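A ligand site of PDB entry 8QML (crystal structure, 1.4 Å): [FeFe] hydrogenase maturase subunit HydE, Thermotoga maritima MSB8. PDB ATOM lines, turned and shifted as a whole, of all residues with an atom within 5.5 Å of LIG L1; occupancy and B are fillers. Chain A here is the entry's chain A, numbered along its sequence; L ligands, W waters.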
ATOM      1  N   CYS A  73     -31.024  -1.007 -13.013  1.00  0.00           N
ATOM      2  CA  CYS A  73     -30.853  -0.251 -11.794  1.00  0.00           C
ATOM      3  C   CYS A  73     -32.145   0.374 -11.372  1.00  0.00           C
ATOM      4  O   CYS A  73     -32.857   0.944 -12.193  1.00  0.00           O
ATOM      5  CB  CYS A  73     -29.873   0.908 -11.980  1.00  0.00           C
ATOM      6  SG  CYS A  73     -29.363   1.549 -10.393  1.00  0.00           S
ATOM      7  N   TYR A  79     -26.076  11.498 -13.116  1.00  0.00           N
ATOM      8  CA  TYR A  79     -24.899  11.357 -13.985  1.00  0.00           C
ATOM      9  C   TYR A  79     -24.837  10.028 -14.718  1.00  0.00           C
ATOM     10  O   TYR A  79     -24.085   9.923 -15.699  1.00  0.00           O
ATOM     11  CB  TYR A  79     -23.632  11.519 -13.129  1.00  0.00           C
ATOM     12  CG  TYR A  79     -23.612  10.744 -11.831  1.00  0.00           C
ATOM     13  CD1 TYR A  79     -23.372   9.396 -11.821  1.00  0.00           C
ATOM     14  CD2 TYR A  79     -23.987  11.382 -10.647  1.00  0.00           C
ATOM     15  CE1 TYR A  79     -23.385   8.619 -10.605  1.00  0.00           C
ATOM     16  CE2 TYR A  79     -24.008  10.673  -9.461  1.00  0.00           C
ATOM     17  CZ  TYR A  79     -23.749   9.324  -9.447  1.00  0.00           C
ATOM     18  OH  TYR A  79     -23.785   8.612  -8.287  1.00  0.00           O
ATOM     19  N   CYS A  80     -25.582   9.012 -14.297  1.00  0.00           N
ATOM     20  CA  CYS A  80     -25.280   7.637 -14.656  1.00  0.00           C
ATOM     21  C   CYS A  80     -26.095   7.160 -15.843  1.00  0.00           C
ATOM     22  O   CYS A  80     -27.325   7.270 -15.825  1.00  0.00           O
ATOM     23  CB  CYS A  80     -25.494   6.696 -13.470  1.00  0.00           C
ATOM     24  SG  CYS A  80     -25.070   5.029 -13.885  1.00  0.00           S
ATOM     25  N   GLY A  81     -25.435   6.579 -16.858  1.00  0.00           N
ATOM     26  CA  GLY A  81     -26.177   6.066 -18.017  1.00  0.00           C
ATOM     27  C   GLY A  81     -27.117   4.901 -17.690  1.00  0.00           C
ATOM     28  O   GLY A  81     -28.026   4.628 -18.488  1.00  0.00           O
ATOM     29  N   GLN A 117     -19.829  -6.198 -10.470  1.00  0.00           N
ATOM     30  CA  GLN A 117     -20.448  -4.881 -10.362  1.00  0.00           C
ATOM     31  C   GLN A 117     -21.754  -4.888 -11.129  1.00  0.00           C
ATOM     32  O   GLN A 117     -21.895  -5.571 -12.143  1.00  0.00           O
ATOM     33  CB  GLN A 117     -19.550  -3.803 -10.936  1.00  0.00           C
ATOM     34  CG  GLN A 117     -20.049  -2.374 -10.640  1.00  0.00           C
ATOM     35  CD  GLN A 117     -19.142  -1.317 -11.171  1.00  0.00           C
ATOM     36  OE1 GLN A 117     -19.113  -1.091 -12.382  1.00  0.00           O
ATOM     37  NE2 GLN A 117     -18.371  -0.679 -10.275  1.00  0.00           N
ATOM     38  N   SER A 118     -22.709  -4.123 -10.647  1.00  0.00           N
ATOM     39  CA  SER A 118     -23.937  -4.048 -11.415  1.00  0.00           C
ATOM     40  C   SER A 118     -24.632  -2.742 -11.027  1.00  0.00           C
ATOM     41  O   SER A 118     -24.255  -2.079 -10.062  1.00  0.00           O
ATOM     42  CB  SER A 118     -24.822  -5.245 -11.027  1.00  0.00           C
ATOM     43  OG  SER A 118     -25.196  -5.175  -9.645  1.00  0.00           O
ATOM     44  N   GLY A 119     -25.685  -2.412 -11.789  1.00  0.00           N
ATOM     45  CA  GLY A 119     -26.687  -1.479 -11.269  1.00  0.00           C
ATOM     46  C   GLY A 119     -27.321  -2.037 -10.008  1.00  0.00           C
ATOM     47  O   GLY A 119     -27.135  -3.199  -9.652  1.00  0.00           O
ATOM     48  N   GLU A 120     -28.084  -1.185  -9.345  1.00  0.00           N
ATOM     49  CA  GLU A 120     -28.808  -1.692  -8.165  1.00  0.00           C
ATOM     50  C   GLU A 120     -29.976  -2.500  -8.692  1.00  0.00           C
ATOM     51  O   GLU A 120     -31.100  -1.997  -8.778  1.00  0.00           O
ATOM     52  CB  GLU A 120     -29.267  -0.579  -7.260  1.00  0.00           C
ATOM     53  CG  GLU A 120     -28.043  -0.014  -6.476  1.00  0.00           C
ATOM     54  CD  GLU A 120     -28.489   0.870  -5.346  1.00  0.00           C
ATOM     55  OE1 GLU A 120     -29.696   0.915  -5.052  1.00  0.00           O
ATOM     56  OE2 GLU A 120     -27.621   1.525  -4.733  1.00  0.00           O
ATOM     57  N   SER A 146     -19.598  -4.722  -5.991  1.00  0.00           N
ATOM     58  CA  SER A 146     -19.855  -3.308  -6.173  1.00  0.00           C
ATOM     59  C   SER A 146     -21.278  -3.250  -6.676  1.00  0.00           C
ATOM     60  O   SER A 146     -21.527  -3.092  -7.866  1.00  0.00           O
ATOM     61  CB  SER A 146     -18.854  -2.770  -7.203  1.00  0.00           C
ATOM     62  OG  SER A 146     -19.028  -1.429  -7.454  1.00  0.00           O
ATOM     63  N   LEU A 147     -22.223  -3.359  -5.736  1.00  0.00           N
ATOM     64  CA  LEU A 147     -23.641  -3.556  -6.084  1.00  0.00           C
ATOM     65  C   LEU A 147     -24.472  -2.385  -5.598  1.00  0.00           C
ATOM     66  O   LEU A 147     -25.678  -2.407  -5.779  1.00  0.00           O
ATOM     67  CB  LEU A 147     -24.183  -4.827  -5.425  1.00  0.00           C
ATOM     68  CG  LEU A 147     -23.276  -6.021  -5.713  1.00  0.00           C
ATOM     69  CD1 LEU A 147     -23.956  -7.289  -5.080  1.00  0.00           C
ATOM     70  CD2 LEU A 147     -22.969  -6.189  -7.196  1.00  0.00           C
ATOM     71  N   GLY A 148     -23.858  -1.352  -5.045  1.00  0.00           N
ATOM     72  CA  GLY A 148     -24.617  -0.204  -4.566  1.00  0.00           C
ATOM     73  C   GLY A 148     -25.034  -0.341  -3.116  1.00  0.00           C
ATOM     74  O   GLY A 148     -24.413  -1.048  -2.303  1.00  0.00           O
ATOM     75  N   LEU A 167     -16.887  -2.194  -3.072  1.00  0.00           N
ATOM     76  CA  LEU A 167     -16.621  -0.871  -3.586  1.00  0.00           C
ATOM     77  C   LEU A 167     -17.909  -0.092  -3.533  1.00  0.00           C
ATOM     78  O   LEU A 167     -18.922  -0.516  -4.110  1.00  0.00           O
ATOM     79  CB  LEU A 167     -16.190  -0.942  -5.035  1.00  0.00           C
ATOM     80  CG  LEU A 167     -15.054  -1.902  -5.343  1.00  0.00           C
ATOM     81  CD1 LEU A 167     -14.807  -1.836  -6.842  1.00  0.00           C
ATOM     82  CD2 LEU A 167     -13.786  -1.459  -4.571  1.00  0.00           C
ATOM     83  N   LEU A 168     -17.857   1.041  -2.869  1.00  0.00           N
ATOM     84  CA  LEU A 168     -19.038   1.906  -2.802  1.00  0.00           C
ATOM     85  C   LEU A 168     -18.527   3.327  -2.785  1.00  0.00           C
ATOM     86  O   LEU A 168     -18.323   3.975  -1.746  1.00  0.00           O
ATOM     87  CB  LEU A 168     -19.881   1.591  -1.577  1.00  0.00           C
ATOM     88  CG  LEU A 168     -21.240   2.283  -1.646  1.00  0.00           C
ATOM     89  CD1 LEU A 168     -22.074   1.568  -2.698  1.00  0.00           C
ATOM     90  CD2 LEU A 168     -21.886   2.078  -0.295  1.00  0.00           C
ATOM     91  N   ARG A 169     -18.223   3.829  -3.978  1.00  0.00           N
ATOM     92  CA  ARG A 169     -17.658   5.179  -4.037  1.00  0.00           C
ATOM     93  C   ARG A 169     -18.582   6.137  -3.356  1.00  0.00           C
ATOM     94  O   ARG A 169     -19.791   6.065  -3.537  1.00  0.00           O
ATOM     95  CB  ARG A 169     -17.544   5.640  -5.449  1.00  0.00           C
ATOM     96  CG  ARG A 169     -16.453   4.896  -6.196  1.00  0.00           C
ATOM     97  CD  ARG A 169     -16.482   5.631  -7.515  1.00  0.00           C
ATOM     98  NE  ARG A 169     -15.505   5.037  -8.390  1.00  0.00           N
ATOM     99  CZ  ARG A 169     -15.083   5.655  -9.475  1.00  0.00           C
ATOM    100  NH1 ARG A 169     -15.741   6.728  -9.954  1.00  0.00           N
ATOM    101  NH2 ARG A 169     -14.019   5.189 -10.101  1.00  0.00           N
ATOM    102  N   GLU A 171     -18.861   9.145  -4.046  1.00  0.00           N
ATOM    103  CA  GLU A 171     -19.287  10.010  -5.159  1.00  0.00           C
ATOM    104  C   GLU A 171     -18.921  11.468  -4.990  1.00  0.00           C
ATOM    105  O   GLU A 171     -18.301  12.084  -5.860  1.00  0.00           O
ATOM    106  CB  GLU A 171     -20.790   9.861  -5.522  1.00  0.00           C
ATOM    107  CG  GLU A 171     -21.170   8.385  -5.550  1.00  0.00           C
ATOM    108  CD  GLU A 171     -20.583   7.580  -6.682  1.00  0.00           C
ATOM    109  OE1 GLU A 171     -19.703   8.067  -7.431  1.00  0.00           O
ATOM    110  OE2 GLU A 171     -21.041   6.432  -6.793  1.00  0.00           O
ATOM    111  N   ARG A 182     -28.105  12.310  -6.695  1.00  0.00           N
ATOM    112  CA  ARG A 182     -28.511  10.935  -6.396  1.00  0.00           C
ATOM    113  C   ARG A 182     -29.835  11.023  -5.664  1.00  0.00           C
ATOM    114  O   ARG A 182     -29.900  10.856  -4.455  1.00  0.00           O
ATOM    115  CB  ARG A 182     -27.450  10.226  -5.573  1.00  0.00           C
ATOM    116  CG  ARG A 182     -26.093  10.390  -6.269  1.00  0.00           C
ATOM    117  CD  ARG A 182     -25.047   9.560  -5.559  1.00  0.00           C
ATOM    118  NE  ARG A 182     -25.303   8.160  -5.783  1.00  0.00           N
ATOM    119  CZ  ARG A 182     -25.626   7.273  -4.866  1.00  0.00           C
ATOM    120  NH1 ARG A 182     -25.563   7.553  -3.567  1.00  0.00           N
ATOM    121  NH2 ARG A 182     -26.057   6.067  -5.249  1.00  0.00           N
ATOM    122  N   ARG A 190     -25.071   6.813   2.047  1.00  0.00           N
ATOM    123  CA  ARG A 190     -23.877   6.284   1.416  1.00  0.00           C
ATOM    124  C   ARG A 190     -22.820   6.039   2.460  1.00  0.00           C
ATOM    125  O   ARG A 190     -22.210   4.978   2.482  1.00  0.00           O
ATOM    126  CB  ARG A 190     -23.321   7.332   0.434  1.00  0.00           C
ATOM    127  CG  ARG A 190     -22.394   6.782  -0.652  1.00  0.00           C
ATOM    128  CD  ARG A 190     -23.139   5.829  -1.549  1.00  0.00           C
ATOM    129  NE  ARG A 190     -22.367   5.587  -2.753  1.00  0.00           N
ATOM    130  CZ  ARG A 190     -22.770   4.760  -3.707  1.00  0.00           C
ATOM    131  NH1 ARG A 190     -24.007   4.250  -3.697  1.00  0.00           N
ATOM    132  NH2 ARG A 190     -21.915   4.434  -4.674  1.00  0.00           N
ATOM    133  N   SER A 208     -14.635   8.922  -5.585  1.00  0.00           N
ATOM    134  CA  SER A 208     -15.529  10.009  -5.972  1.00  0.00           C
ATOM    135  C   SER A 208     -15.252  10.359  -7.409  1.00  0.00           C
ATOM    136  O   SER A 208     -14.206   9.999  -7.969  1.00  0.00           O
ATOM    137  CB  SER A 208     -15.337  11.241  -5.080  1.00  0.00           C
ATOM    138  OG  SER A 208     -13.924  11.577  -4.974  1.00  0.00           O
ATOM    139  N   MET A 209     -16.178  11.089  -8.007  1.00  0.00           N
ATOM    140  CA  MET A 209     -15.956  11.639  -9.316  1.00  0.00           C
ATOM    141  C   MET A 209     -15.421  13.037  -9.186  1.00  0.00           C
ATOM    142  O   MET A 209     -15.696  13.756  -8.232  1.00  0.00           O
ATOM    143  CB  MET A 209     -17.270  11.681 -10.124  1.00  0.00           C
ATOM    144  CG  MET A 209     -17.642  10.298 -10.600  1.00  0.00           C
ATOM    145  SD  MET A 209     -19.308  10.269 -11.332  1.00  0.00           S
ATOM    146  CE  MET A 209     -20.304  10.369  -9.832  1.00  0.00           C
ATOM    147  N   PRO A 239     -12.859  10.947 -13.536  1.00  0.00           N
ATOM    148  CA  PRO A 239     -13.589  12.141 -13.930  1.00  0.00           C
ATOM    149  C   PRO A 239     -15.046  11.790 -14.071  1.00  0.00           C
ATOM    150  O   PRO A 239     -15.400  10.641 -14.319  1.00  0.00           O
ATOM    151  CB  PRO A 239     -13.017  12.462 -15.322  1.00  0.00           C
ATOM    152  CG  PRO A 239     -12.648  11.021 -15.862  1.00  0.00           C
ATOM    153  CD  PRO A 239     -12.061  10.340 -14.623  1.00  0.00           C
ATOM    154  N   PHE A 240     -15.877  12.798 -13.867  1.00  0.00           N
ATOM    155  CA  PHE A 240     -17.223  12.727 -14.395  1.00  0.00           C
ATOM    156  C   PHE A 240     -17.187  12.779 -15.918  1.00  0.00           C
ATOM    157  O   PHE A 240     -16.543  13.634 -16.498  1.00  0.00           O
ATOM    158  CB  PHE A 240     -18.002  13.886 -13.825  1.00  0.00           C
ATOM    159  CG  PHE A 240     -19.289  14.189 -14.566  1.00  0.00           C
ATOM    160  CD1 PHE A 240     -20.344  13.248 -14.606  1.00  0.00           C
ATOM    161  CD2 PHE A 240     -19.388  15.346 -15.253  1.00  0.00           C
ATOM    162  CE1 PHE A 240     -21.502  13.495 -15.345  1.00  0.00           C
ATOM    163  CE2 PHE A 240     -20.570  15.627 -15.971  1.00  0.00           C
ATOM    164  CZ  PHE A 240     -21.595  14.683 -16.004  1.00  0.00           C
ATOM    165  N   ILE A 241     -17.910  11.886 -16.575  1.00  0.00           N
ATOM    166  CA  ILE A 241     -17.992  11.862 -18.017  1.00  0.00           C
ATOM    167  C   ILE A 241     -19.471  11.986 -18.349  1.00  0.00           C
ATOM    168  O   ILE A 241     -20.250  11.104 -17.951  1.00  0.00           O
ATOM    169  CB  ILE A 241     -17.382  10.573 -18.614  1.00  0.00           C
ATOM    170  CG1 ILE A 241     -15.872  10.513 -18.354  1.00  0.00           C
ATOM    171  CG2 ILE A 241     -17.480  10.631 -20.138  1.00  0.00           C
ATOM    172  CD1 ILE A 241     -15.295   9.180 -18.598  1.00  0.00           C
ATOM    173  N   PRO A 242     -19.909  13.045 -19.026  1.00  0.00           N
ATOM    174  CA  PRO A 242     -21.348  13.209 -19.293  1.00  0.00           C
ATOM    175  C   PRO A 242     -21.897  12.137 -20.230  1.00  0.00           C
ATOM    176  O   PRO A 242     -21.262  11.745 -21.206  1.00  0.00           O
ATOM    177  CB  PRO A 242     -21.436  14.590 -19.950  1.00  0.00           C
ATOM    178  CG  PRO A 242     -20.028  14.829 -20.529  1.00  0.00           C
ATOM    179  CD  PRO A 242     -19.121  14.201 -19.500  1.00  0.00           C
ATOM    180  N   HIS A 243     -23.125  11.676 -19.933  1.00  0.00           N
ATOM    181  CA  HIS A 243     -23.718  10.654 -20.750  1.00  0.00           C
ATOM    182  C   HIS A 243     -24.908  11.289 -21.444  1.00  0.00           C
ATOM    183  O   HIS A 243     -25.724  11.968 -20.792  1.00  0.00           O
ATOM    184  CB  HIS A 243     -24.179   9.494 -19.869  1.00  0.00           C
ATOM    185  CG  HIS A 243     -24.638   8.279 -20.625  1.00  0.00           C
ATOM    186  ND1 HIS A 243     -25.757   8.277 -21.442  1.00  0.00           N
ATOM    187  CD2 HIS A 243     -24.142   7.018 -20.668  1.00  0.00           C
ATOM    188  CE1 HIS A 243     -25.918   7.074 -21.965  1.00  0.00           C
ATOM    189  NE2 HIS A 243     -24.939   6.298 -21.528  1.00  0.00           N
ATOM    190  N   ALA A 280     -12.376   5.173 -16.398  1.00  0.00           N
ATOM    191  CA  ALA A 280     -12.785   6.515 -16.793  1.00  0.00           C
ATOM    192  C   ALA A 280     -11.566   7.357 -17.099  1.00  0.00           C
ATOM    193  O   ALA A 280     -11.585   8.163 -18.034  1.00  0.00           O
ATOM    194  CB  ALA A 280     -13.603   7.179 -15.690  1.00  0.00           C
ATOM    195  N   TYR A 313     -23.193  -1.877 -20.870  1.00  0.00           N
ATOM    196  CA  TYR A 313     -22.958  -1.377 -19.526  1.00  0.00           C
ATOM    197  C   TYR A 313     -22.254  -0.046 -19.663  1.00  0.00           C
ATOM    198  O   TYR A 313     -21.037   0.041 -19.596  1.00  0.00           O
ATOM    199  CB  TYR A 313     -22.180  -2.394 -18.697  1.00  0.00           C
ATOM    200  CG  TYR A 313     -22.118  -2.077 -17.248  1.00  0.00           C
ATOM    201  CD1 TYR A 313     -23.089  -2.575 -16.375  1.00  0.00           C
ATOM    202  CD2 TYR A 313     -21.101  -1.314 -16.747  1.00  0.00           C
ATOM    203  CE1 TYR A 313     -23.049  -2.301 -15.023  1.00  0.00           C
ATOM    204  CE2 TYR A 313     -21.009  -1.043 -15.398  1.00  0.00           C
ATOM    205  CZ  TYR A 313     -21.987  -1.559 -14.551  1.00  0.00           C
ATOM    206  OH  TYR A 313     -21.910  -1.310 -13.186  1.00  0.00           O
ATOM    207  N   LEU A 315     -22.011   3.244 -18.139  1.00  0.00           N
ATOM    208  CA  LEU A 315     -22.180   4.286 -17.129  1.00  0.00           C
ATOM    209  C   LEU A 315     -21.933   5.650 -17.730  1.00  0.00           C
ATOM    210  O   LEU A 315     -22.614   6.637 -17.420  1.00  0.00           O
ATOM    211  CB  LEU A 315     -21.121   4.077 -16.036  1.00  0.00           C
ATOM    212  CG  LEU A 315     -21.105   2.712 -15.416  1.00  0.00           C
ATOM    213  CD1 LEU A 315     -19.883   2.650 -14.530  1.00  0.00           C
ATOM    214  CD2 LEU A 315     -22.389   2.659 -14.551  1.00  0.00           C
ATOM    215  N   TYR A 316     -20.934   5.739 -18.593  1.00  0.00           N
ATOM    216  CA  TYR A 316     -20.672   6.931 -19.364  1.00  0.00           C
ATOM    217  C   TYR A 316     -20.250   6.444 -20.740  1.00  0.00           C
ATOM    218  O   TYR A 316     -19.894   5.263 -20.909  1.00  0.00           O
ATOM    219  CB  TYR A 316     -19.524   7.730 -18.704  1.00  0.00           C
ATOM    220  CG  TYR A 316     -18.339   6.859 -18.390  1.00  0.00           C
ATOM    221  CD1 TYR A 316     -17.397   6.552 -19.371  1.00  0.00           C
ATOM    222  CD2 TYR A 316     -18.161   6.308 -17.117  1.00  0.00           C
ATOM    223  CE1 TYR A 316     -16.333   5.720 -19.096  1.00  0.00           C
ATOM    224  CE2 TYR A 316     -17.131   5.483 -16.827  1.00  0.00           C
ATOM    225  CZ  TYR A 316     -16.173   5.179 -17.833  1.00  0.00           C
ATOM    226  OH  TYR A 316     -15.109   4.367 -17.549  1.00  0.00           O
HETATM  227  N1  LIG L   1     -24.559   0.767  -8.866  1.00  0.00           N
HETATM  228  C1  LIG L   1     -23.261   0.739  -8.164  1.00  0.00           C
HETATM  229  C2  LIG L   1     -22.114   0.236  -9.031  1.00  0.00           C
HETATM  230  C3  LIG L   1     -22.028   0.753 -10.479  1.00  0.00           C
HETATM  231  S1  LIG L   1     -21.744   2.536 -10.687  1.00  0.00           S
HETATM  232  C4  LIG L   1     -22.991   2.053  -7.492  1.00  0.00           C
HETATM  233  O1  LIG L   1     -23.622   3.093  -7.786  1.00  0.00           O
HETATM  234  O2  LIG L   1     -22.139   2.064  -6.585  1.00  0.00           O
HETATM  235  C5  LIG L   1     -19.950   2.561 -10.422  1.00  0.00           C
HETATM  236  C6  LIG L   1     -19.345   3.978 -10.412  1.00  0.00           C
HETATM  237  O3  LIG L   1     -19.413   4.514 -11.720  1.00  0.00           O
HETATM  238  C7  LIG L   1     -20.142   4.984  -9.593  1.00  0.00           C
HETATM  239  O4  LIG L   1     -19.723   4.839  -8.244  1.00  0.00           O
HETATM  240  C8  LIG L   1     -19.755   6.310 -10.232  1.00  0.00           C
HETATM  241  O5  LIG L   1     -18.741   7.016  -9.519  1.00  0.00           O
HETATM  242  C9  LIG L   1     -19.231   5.899 -11.625  1.00  0.00           C
HETATM  243  N2  LIG L   1     -19.974   6.585 -12.674  1.00  0.00           N
HETATM  244  C10 LIG L   1     -21.368   6.527 -12.898  1.00  0.00           C
HETATM  245  N3  LIG L   1     -21.684   7.348 -13.880  1.00  0.00           N
HETATM  246  C11 LIG L   1     -20.530   8.005 -14.281  1.00  0.00           C
HETATM  247  C12 LIG L   1     -20.277   8.955 -15.273  1.00  0.00           C
HETATM  248  N4  LIG L   1     -21.238   9.490 -16.056  1.00  0.00           N
HETATM  249  N5  LIG L   1     -18.997   9.425 -15.439  1.00  0.00           N
HETATM  250  C13 LIG L   1     -17.971   8.937 -14.657  1.00  0.00           C
HETATM  251  N6  LIG L   1     -18.187   7.968 -13.695  1.00  0.00           N
HETATM  252  C14 LIG L   1     -19.471   7.516 -13.506  1.00  0.00           C
HETATM  253 FE1  LG2 L   2     -25.725   4.240 -11.938  1.00  0.00          FE
HETATM  254 FE2  LG2 L   2     -27.587   2.875 -10.582  1.00  0.00          FE
HETATM  255 FE3  LG2 L   2     -26.626   5.241  -9.594  1.00  0.00          FE
HETATM  256 FE4  LG2 L   2     -24.952   2.927  -9.580  1.00  0.00          FE
HETATM  257  S1  LG2 L   2     -26.936   3.328  -8.420  1.00  0.00           S
HETATM  258  S2  LG2 L   2     -24.438   5.087 -10.258  1.00  0.00           S
HETATM  259  S3  LG2 L   2     -25.752   2.003 -11.569  1.00  0.00           S
HETATM  260  S4  LG2 L   2     -27.859   4.941 -11.497  1.00  0.00           S
HETATM  261  O1  LG3 L   3     -13.681   0.839  -8.881  1.00  0.00           O
HETATM  262  C1  LG3 L   3     -13.656   1.672  -9.817  1.00  0.00           C
HETATM  263  O2  LG3 L   3     -12.922   2.701  -9.785  1.00  0.00           O
HETATM  264  C2  LG3 L   3     -14.551   1.376 -10.995  1.00  0.00           C
HETATM  265  C3  LG3 L   3     -14.669  -0.150 -11.238  1.00  0.00           C
HETATM  266  N1  LG3 L   3     -13.982   2.033 -12.165  1.00  0.00           N
HETATM  267  S1  LG3 L   3     -16.169   2.094 -10.779  1.00  0.00           S
HETATM  268  C4  LG3 L   3     -16.233   2.999 -12.292  1.00  0.00           C
HETATM  269  C5  LG3 L   3     -15.092   2.338 -13.098  1.00  0.00           C
HETATM  270  C6  LG3 L   3     -14.693   3.196 -14.263  1.00  0.00           C
HETATM  271  O3  LG3 L   3     -13.762   4.003 -14.137  1.00  0.00           O
HETATM  272  O4  LG3 L   3     -15.307   3.115 -15.335  1.00  0.00           O
HETATM  273  O   HOH W   1     -23.638   5.997  -7.378  1.00  0.00           O
HETATM  274  O   HOH W   2     -21.044  -0.353  -5.653  1.00  0.00           O
HETATM  275  O   HOH W   3     -19.460   2.847  -6.459  1.00  0.00           O
HETATM  276  O   HOH W   4     -15.541   8.161 -12.739  1.00  0.00           O
HETATM  277  O   HOH W   5     -25.513   2.900  -5.539  1.00  0.00           O
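An oxygen (O1) of LIG L1 is bound to an iron atom (FE4) of LG2 L2 (2.2 Å).
N4 of LIG L1 lies within hydrogen-bond range of O of Ile 241 (2.7 Å).
O of Ser 118 lies close to N1 of LIG L1, at 3.1 Å.
An iron atom (FE2) of LG2 L2 is bound by the side-chain sulfur (SG) of Cys 73, at 2.2 Å.
A sulfur (S1) of LG3 L3 lies close to the side-chain amide nitrogen (NE2) of Gln 117.
O3 of LG3 L3 is in hydrogen-bond range of N of Ala 280 (2.9 Å).
NH2 of Arg 190 is in salt-bridge range of O2 of LIG L1, at 3.1 Å.
FE1 of LG2 L2 is bound by SG of Cys 80, 2.2 Å away.
OE2 of Glu 171 is in hydrogen-bond range of O4 of LIG L1 (2.5 Å).
O5 of LIG L1 lies within hydrogen-bond range of NH1 of Arg 169 (3.0 Å).
O of Leu 315 lies within hydrogen-bond range of N4 of LIG L1 (3.4 Å).
NH2 of Arg 169 is in salt-bridge range of O2 of LG3 L3 (2.7 Å).
A nitrogen (N5) of LIG L1 lies within hydrogen-bond range of the backbone NH (N) of Ile 241.
The side-chain hydroxyl of Tyr 316 lies within hydrogen-bond range of an oxygen (O4) of LG3 L3, 2.6 Å away.
O of Tyr 79 lies within hydrogen-bond range of N4 of LIG L1, 2.9 Å away.
O5 of LIG L1 lies close to SD of Met 209 (3.8 Å).
The backbone carbonyl oxygen of Arg 169 lies within hydrogen-bond range of the guanidinium group of Arg 190, 2.7 Å away.
The side-chain hydroxyl of Tyr 313 lies within hydrogen-bond range of the side-chain amide oxygen of Gln 117, 2.9 Å away.
OH of Tyr 79 sits at hydrogen-bond distance from NE of Arg 182 (3.0 Å).
The side-chain hydroxyl of Tyr 316 is in hydrogen-bond range of the backbone NH of Ala 280 (3.1 Å).
The side-chain hydroxyl (OG) of Ser 146 sits at hydrogen-bond distance from the backbone carbonyl oxygen (O) of Leu 167.
O of Ser 146 lies within hydrogen-bond range of N of Ser 118 (3.2 Å).
The backbone carbonyl oxygen (O) of Leu 315 sits at hydrogen-bond distance from the backbone NH (N) of Gly 81 (2.9 Å).
OE2 of Glu 171 is in salt-bridge range of NH2 of Arg 190 (3.0 Å).
Water W3 lies within hydrogen-bond range of O4 of LIG L1, N of Arg 169 and NH2 of Arg 190.
Water W2 lies within hydrogen-bond range of O of Leu 167 (2.6 Å), O2 of LIG L1 (2.8 Å), OG of Ser 146 (2.9 Å), N of Gly 148 (3.0 Å) and N of Leu 147 (3.2 Å).
Water W4 lies within hydrogen-bond range of a nitrogen (N6) of LIG L1 (2.8 Å), the backbone carbonyl oxygen of Pro 239 (2.9 Å) and the guanidinium group of Arg 169 (3.1 Å).
Water W1 lies within hydrogen-bond range of the side-chain carboxylate of Glu 171 (2.7 Å), the side-chain hydroxyl of Tyr 79 (2.8 Å), a sulfur (S2) of LG2 L2 (3.1 Å) and the guanidinium group of Arg 182 (3.2 Å).
Water W5 lies within hydrogen-bond range of the side-chain carboxylate (OE2) of Glu 120, the guanidinium group (NH1) of Arg 190, the guanidinium group (NH2) of Arg 182 and a sulfur (S1) of LG2 L2.
Merely in contact with LIG L1: Pro 239 (3.1 Å), Tyr 313 (3.4 Å), Ser 146 (3.6 Å), Tyr 316 (3.6 Å), Gln 117 (3.6 Å), Cys 80 (3.7 Å), Gly 148 (3.8 Å), Phe 240 (3.8 Å), Gly 119 (3.9 Å) and Leu 168 (3.9 Å).
Hydrophobic or aromatic side chains that line LIG L1: Tyr 79, Leu 168, Met 209, Ile 241, Leu 315 and Tyr 316.
The nearest printed residue that does not touch LIG L1 is Glu 120 (4.1 Å).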
